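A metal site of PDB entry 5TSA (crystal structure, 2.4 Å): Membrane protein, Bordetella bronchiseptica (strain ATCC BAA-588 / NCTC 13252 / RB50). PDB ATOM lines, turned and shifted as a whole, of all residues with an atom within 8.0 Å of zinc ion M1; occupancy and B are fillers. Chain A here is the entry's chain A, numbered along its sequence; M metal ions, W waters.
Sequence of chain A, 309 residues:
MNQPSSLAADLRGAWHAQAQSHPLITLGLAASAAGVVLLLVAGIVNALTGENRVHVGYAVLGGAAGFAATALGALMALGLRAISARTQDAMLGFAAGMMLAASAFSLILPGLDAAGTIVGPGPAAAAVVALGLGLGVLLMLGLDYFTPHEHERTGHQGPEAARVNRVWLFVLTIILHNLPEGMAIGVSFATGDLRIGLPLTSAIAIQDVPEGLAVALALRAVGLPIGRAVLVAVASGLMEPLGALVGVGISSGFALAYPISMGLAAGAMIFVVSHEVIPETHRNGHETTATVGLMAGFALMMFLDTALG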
ATOM      1  N   LEU A  92      17.525  33.168 -10.162  1.00  0.00           N
ATOM      2  CA  LEU A  92      17.270  31.918 -10.848  1.00  0.00           C
ATOM      3  C   LEU A  92      18.267  30.842 -10.424  1.00  0.00           C
ATOM      4  O   LEU A  92      17.895  29.672 -10.295  1.00  0.00           O
ATOM      5  CB  LEU A  92      17.286  32.147 -12.357  1.00  0.00           C
ATOM      6  CG  LEU A  92      16.227  33.173 -12.813  1.00  0.00           C
ATOM      7  CD1 LEU A  92      16.398  33.531 -14.277  1.00  0.00           C
ATOM      8  CD2 LEU A  92      14.825  32.654 -12.542  1.00  0.00           C
ATOM      9  N   PHE A  94      19.632  30.757  -7.449  1.00  0.00           N
ATOM     10  CA  PHE A  94      19.143  30.377  -6.132  1.00  0.00           C
ATOM     11  C   PHE A  94      17.969  29.413  -6.228  1.00  0.00           C
ATOM     12  O   PHE A  94      17.930  28.412  -5.502  1.00  0.00           O
ATOM     13  CB  PHE A  94      18.772  31.628  -5.360  1.00  0.00           C
ATOM     14  CG  PHE A  94      18.093  31.375  -4.049  1.00  0.00           C
ATOM     15  CD1 PHE A  94      18.831  31.095  -2.915  1.00  0.00           C
ATOM     16  CD2 PHE A  94      16.701  31.469  -3.943  1.00  0.00           C
ATOM     17  CE1 PHE A  94      18.199  30.892  -1.693  1.00  0.00           C
ATOM     18  CE2 PHE A  94      16.069  31.274  -2.739  1.00  0.00           C
ATOM     19  CZ  PHE A  94      16.816  30.990  -1.606  1.00  0.00           C
ATOM     20  N   ALA A  95      17.023  29.669  -7.139  1.00  0.00           N
ATOM     21  CA  ALA A  95      15.880  28.771  -7.283  1.00  0.00           C
ATOM     22  C   ALA A  95      16.326  27.382  -7.723  1.00  0.00           C
ATOM     23  O   ALA A  95      15.879  26.366  -7.163  1.00  0.00           O
ATOM     24  CB  ALA A  95      14.856  29.344  -8.270  1.00  0.00           C
ATOM     25  N   ALA A  96      17.224  27.320  -8.718  1.00  0.00           N
ATOM     26  CA  ALA A  96      17.744  26.047  -9.206  1.00  0.00           C
ATOM     27  C   ALA A  96      18.468  25.289  -8.099  1.00  0.00           C
ATOM     28  O   ALA A  96      18.267  24.081  -7.924  1.00  0.00           O
ATOM     29  CB  ALA A  96      18.675  26.305 -10.387  1.00  0.00           C
ATOM     30  N   GLY A  97      19.319  25.986  -7.341  1.00  0.00           N
ATOM     31  CA  GLY A  97      20.077  25.334  -6.296  1.00  0.00           C
ATOM     32  C   GLY A  97      19.192  24.723  -5.220  1.00  0.00           C
ATOM     33  O   GLY A  97      19.510  23.663  -4.679  1.00  0.00           O
ATOM     34  N   MET A  98      18.077  25.385  -4.918  1.00  0.00           N
ATOM     35  CA  MET A  98      17.145  24.878  -3.914  1.00  0.00           C
ATOM     36  C   MET A  98      16.476  23.588  -4.371  1.00  0.00           C
ATOM     37  O   MET A  98      16.266  22.666  -3.564  1.00  0.00           O
ATOM     38  CB  MET A  98      16.091  25.934  -3.613  1.00  0.00           C
ATOM     39  CG  MET A  98      16.625  27.148  -2.849  1.00  0.00           C
ATOM     40  SD  MET A  98      16.237  27.019  -1.093  1.00  0.00           S
ATOM     41  CE  MET A  98      14.584  27.651  -1.125  1.00  0.00           C
ATOM     42  N   MET A  99      16.092  23.524  -5.643  1.00  0.00           N
ATOM     43  CA  MET A  99      15.385  22.364  -6.128  1.00  0.00           C
ATOM     44  C   MET A  99      16.334  21.213  -6.416  1.00  0.00           C
ATOM     45  O   MET A  99      15.948  20.051  -6.261  1.00  0.00           O
ATOM     46  CB  MET A  99      14.573  22.753  -7.366  1.00  0.00           C
ATOM     47  CG  MET A  99      13.309  23.560  -7.019  1.00  0.00           C
ATOM     48  SD  MET A  99      12.517  23.187  -5.411  1.00  0.00           S
ATOM     49  CE  MET A  99      12.060  21.452  -5.522  1.00  0.00           C
ATOM     50  N   LEU A 100      17.587  21.509  -6.773  1.00  0.00           N
ATOM     51  CA  LEU A 100      18.575  20.457  -6.974  1.00  0.00           C
ATOM     52  C   LEU A 100      18.839  19.718  -5.664  1.00  0.00           C
ATOM     53  O   LEU A 100      18.803  18.472  -5.629  1.00  0.00           O
ATOM     54  CB  LEU A 100      19.862  21.051  -7.527  1.00  0.00           C
ATOM     55  CG  LEU A 100      19.673  21.039  -9.041  1.00  0.00           C
ATOM     56  CD1 LEU A 100      20.517  22.087  -9.736  1.00  0.00           C
ATOM     57  CD2 LEU A 100      19.935  19.635  -9.585  1.00  0.00           C
ATOM     58  N   HIS A 177       7.311  23.933 -15.996  1.00  0.00           N
ATOM     59  CA  HIS A 177       8.365  23.931 -14.994  1.00  0.00           C
ATOM     60  C   HIS A 177       7.801  23.999 -13.586  1.00  0.00           C
ATOM     61  O   HIS A 177       8.477  23.591 -12.639  1.00  0.00           O
ATOM     62  CB  HIS A 177       9.331  25.092 -15.290  1.00  0.00           C
ATOM     63  CG  HIS A 177      10.185  24.862 -16.512  1.00  0.00           C
ATOM     64  ND1 HIS A 177      11.187  25.716 -16.901  1.00  0.00           N
ATOM     65  CD2 HIS A 177      10.178  23.861 -17.430  1.00  0.00           C
ATOM     66  CE1 HIS A 177      11.760  25.265 -17.998  1.00  0.00           C
ATOM     67  NE2 HIS A 177      11.160  24.131 -18.342  1.00  0.00           N
ATOM     68  N   ASN A 178       6.555  24.455 -13.429  1.00  0.00           N
ATOM     69  CA  ASN A 178       5.859  24.381 -12.148  1.00  0.00           C
ATOM     70  C   ASN A 178       5.327  22.988 -11.843  1.00  0.00           C
ATOM     71  O   ASN A 178       5.117  22.678 -10.663  1.00  0.00           O
ATOM     72  CB  ASN A 178       4.679  25.357 -12.122  1.00  0.00           C
ATOM     73  CG  ASN A 178       5.112  26.781 -11.853  1.00  0.00           C
ATOM     74  OD1 ASN A 178       6.172  27.005 -11.288  1.00  0.00           O
ATOM     75  ND2 ASN A 178       4.304  27.755 -12.272  1.00  0.00           N
ATOM     76  N   GLU A 181       7.335  20.791  -9.251  1.00  0.00           N
ATOM     77  CA  GLU A 181       7.321  21.330  -7.892  1.00  0.00           C
ATOM     78  C   GLU A 181       5.976  21.073  -7.209  1.00  0.00           C
ATOM     79  O   GLU A 181       5.937  20.677  -6.038  1.00  0.00           O
ATOM     80  CB  GLU A 181       7.666  22.826  -7.930  1.00  0.00           C
ATOM     81  CG  GLU A 181       9.164  23.004  -8.147  1.00  0.00           C
ATOM     82  CD  GLU A 181       9.557  24.379  -8.601  1.00  0.00           C
ATOM     83  OE1 GLU A 181       8.687  25.221  -8.617  1.00  0.00           O
ATOM     84  OE2 GLU A 181      10.735  24.620  -8.939  1.00  0.00           O
ATOM     85  N   ALA A 203      10.811  24.951   1.274  1.00  0.00           N
ATOM     86  CA  ALA A 203      11.854  25.292   0.293  1.00  0.00           C
ATOM     87  C   ALA A 203      11.242  25.705  -1.046  1.00  0.00           C
ATOM     88  O   ALA A 203      11.744  26.616  -1.709  1.00  0.00           O
ATOM     89  CB  ALA A 203      12.786  24.108   0.101  1.00  0.00           C
ATOM     90  N   ILE A 204      10.164  25.036  -1.460  1.00  0.00           N
ATOM     91  CA  ILE A 204       9.559  25.344  -2.759  1.00  0.00           C
ATOM     92  C   ILE A 204       8.886  26.708  -2.709  1.00  0.00           C
ATOM     93  O   ILE A 204       9.009  27.514  -3.644  1.00  0.00           O
ATOM     94  CB  ILE A 204       8.592  24.216  -3.172  1.00  0.00           C
ATOM     95  CG1 ILE A 204       9.388  23.001  -3.683  1.00  0.00           C
ATOM     96  CG2 ILE A 204       7.575  24.655  -4.220  1.00  0.00           C
ATOM     97  CD1 ILE A 204       8.532  21.748  -3.999  1.00  0.00           C
ATOM     98  N   GLN A 207      11.712  29.465  -2.911  1.00  0.00           N
ATOM     99  CA  GLN A 207      12.188  29.825  -4.248  1.00  0.00           C
ATOM    100  C   GLN A 207      11.060  30.241  -5.195  1.00  0.00           C
ATOM    101  O   GLN A 207      11.361  30.765  -6.280  1.00  0.00           O
ATOM    102  CB  GLN A 207      13.004  28.687  -4.877  1.00  0.00           C
ATOM    103  CG  GLN A 207      12.362  27.296  -4.942  1.00  0.00           C
ATOM    104  CD  GLN A 207      11.561  27.045  -6.225  1.00  0.00           C
ATOM    105  OE1 GLN A 207      12.128  26.715  -7.290  1.00  0.00           O
ATOM    106  NE2 GLN A 207      10.228  27.143  -6.117  1.00  0.00           N
ATOM    107  N   ASP A 208       9.792  30.031  -4.820  1.00  0.00           N
ATOM    108  CA  ASP A 208       8.677  30.533  -5.620  1.00  0.00           C
ATOM    109  C   ASP A 208       8.609  32.055  -5.662  1.00  0.00           C
ATOM    110  O   ASP A 208       8.140  32.626  -6.648  1.00  0.00           O
ATOM    111  CB  ASP A 208       7.348  30.024  -5.071  1.00  0.00           C
ATOM    112  CG  ASP A 208       7.001  28.666  -5.596  1.00  0.00           C
ATOM    113  OD1 ASP A 208       7.755  28.185  -6.457  1.00  0.00           O
ATOM    114  OD2 ASP A 208       6.009  28.077  -5.132  1.00  0.00           O
ATOM    115  N   GLU A 211      10.937  33.207  -8.184  1.00  0.00           N
ATOM    116  CA  GLU A 211      10.512  32.676  -9.477  1.00  0.00           C
ATOM    117  C   GLU A 211       9.275  33.393  -9.981  1.00  0.00           C
ATOM    118  O   GLU A 211       9.185  33.685 -11.175  1.00  0.00           O
ATOM    119  CB  GLU A 211      10.253  31.173  -9.389  1.00  0.00           C
ATOM    120  CG  GLU A 211      11.542  30.351  -9.425  1.00  0.00           C
ATOM    121  CD  GLU A 211      11.253  28.908  -9.660  1.00  0.00           C
ATOM    122  OE1 GLU A 211      10.117  28.517  -9.335  1.00  0.00           O
ATOM    123  OE2 GLU A 211      12.112  28.176 -10.186  1.00  0.00           O
ATOM    124  N   GLU A 240       1.000  24.663  -9.101  1.00  0.00           N
ATOM    125  CA  GLU A 240       1.487  23.941  -7.930  1.00  0.00           C
ATOM    126  C   GLU A 240       0.341  23.304  -7.146  1.00  0.00           C
ATOM    127  O   GLU A 240       0.467  22.135  -6.761  1.00  0.00           O
ATOM    128  CB  GLU A 240       2.326  24.859  -7.051  1.00  0.00           C
ATOM    129  CG  GLU A 240       3.127  25.779  -7.955  1.00  0.00           C
ATOM    130  CD  GLU A 240       4.483  26.179  -7.403  1.00  0.00           C
ATOM    131  OE1 GLU A 240       4.711  26.188  -6.176  1.00  0.00           O
ATOM    132  OE2 GLU A 240       5.326  26.480  -8.245  1.00  0.00           O
ATOM    133  N   MET A 269      11.882  16.947 -11.518  1.00  0.00           N
ATOM    134  CA  MET A 269      12.509  18.135 -10.943  1.00  0.00           C
ATOM    135  C   MET A 269      13.919  18.356 -11.511  1.00  0.00           C
ATOM    136  O   MET A 269      14.313  19.498 -11.796  1.00  0.00           O
ATOM    137  CB  MET A 269      12.559  17.977  -9.426  1.00  0.00           C
ATOM    138  CG  MET A 269      12.869  19.224  -8.632  1.00  0.00           C
ATOM    139  SD  MET A 269      11.372  20.205  -8.489  1.00  0.00           S
ATOM    140  CE  MET A 269      11.672  21.386  -9.828  1.00  0.00           C
ATOM    141  N   VAL A 272      13.775  19.708 -15.166  1.00  0.00           N
ATOM    142  CA  VAL A 272      13.414  21.114 -15.255  1.00  0.00           C
ATOM    143  C   VAL A 272      14.609  21.993 -14.881  1.00  0.00           C
ATOM    144  O   VAL A 272      14.940  22.942 -15.590  1.00  0.00           O
ATOM    145  CB  VAL A 272      12.185  21.419 -14.389  1.00  0.00           C
ATOM    146  CG1 VAL A 272      12.084  22.920 -14.177  1.00  0.00           C
ATOM    147  CG2 VAL A 272      10.950  20.923 -15.062  1.00  0.00           C
ATOM    148  N   VAL A 273      15.320  21.650 -13.796  1.00  0.00           N
ATOM    149  CA  VAL A 273      16.377  22.555 -13.342  1.00  0.00           C
ATOM    150  C   VAL A 273      17.611  22.479 -14.238  1.00  0.00           C
ATOM    151  O   VAL A 273      18.289  23.492 -14.431  1.00  0.00           O
ATOM    152  CB  VAL A 273      16.714  22.284 -11.858  1.00  0.00           C
ATOM    153  CG1 VAL A 273      15.461  22.389 -11.004  1.00  0.00           C
ATOM    154  CG2 VAL A 273      17.321  20.943 -11.688  1.00  0.00           C
ATOM    155  N   GLU A 276      17.019  25.049 -16.729  1.00  0.00           N
ATOM    156  CA  GLU A 276      17.097  26.414 -16.229  1.00  0.00           C
ATOM    157  C   GLU A 276      18.507  26.782 -15.779  1.00  0.00           C
ATOM    158  O   GLU A 276      18.736  27.917 -15.352  1.00  0.00           O
ATOM    159  CB  GLU A 276      16.095  26.596 -15.081  1.00  0.00           C
ATOM    160  CG  GLU A 276      14.651  26.183 -15.441  1.00  0.00           C
ATOM    161  CD  GLU A 276      13.633  26.508 -14.350  1.00  0.00           C
ATOM    162  OE1 GLU A 276      13.898  26.162 -13.161  1.00  0.00           O
ATOM    163  OE2 GLU A 276      12.569  27.109 -14.689  1.00  0.00           O
HETATM  164 ZN    ZN M   1      11.776  26.300  -9.376  1.00  0.00          ZN
HETATM  165 CD    CD M   2       7.569  27.553  -9.049  1.00  0.00          CD
HETATM  166 ZN    ZN M   3      11.622  27.619 -16.397  1.00  0.00          ZN
HETATM  167  O   HOH W   1      13.748  25.752  -9.530  1.00  0.00           O
HETATM  168  O   HOH W   2      11.308  25.993 -11.817  1.00  0.00           O
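The side-chain carboxylate of Asp 208 sits at hydrogen-bond distance from the side-chain amide nitrogen of Gln 207, 2.7 Å away. The backbone carbonyl oxygen (O) of Ile 204 is in hydrogen-bond range of the side-chain amide nitrogen (NE2) of Gln 207 (2.8 Å).
Zinc ion M1 is bound by OE2 of Glu 181 (2.0 Å). Water W1 binds zinc ion M1, at 2.1 Å. The side-chain carboxylate (OE2) of Glu 211 binds zinc ion M1, at 2.1 Å. The side-chain amide oxygen (OE1) of Gln 207 is bound to zinc ion M1 (2.2 Å). Water W2 is bound to zinc ion M1 (2.5 Å). Zinc ion M1 has five donor atoms within binding distance. Slightly farther from zinc ion M1 lies OE1 of Glu 211 (2.8 Å).
CG of Met 99 touches zinc ion M1, 3.9 Å away.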
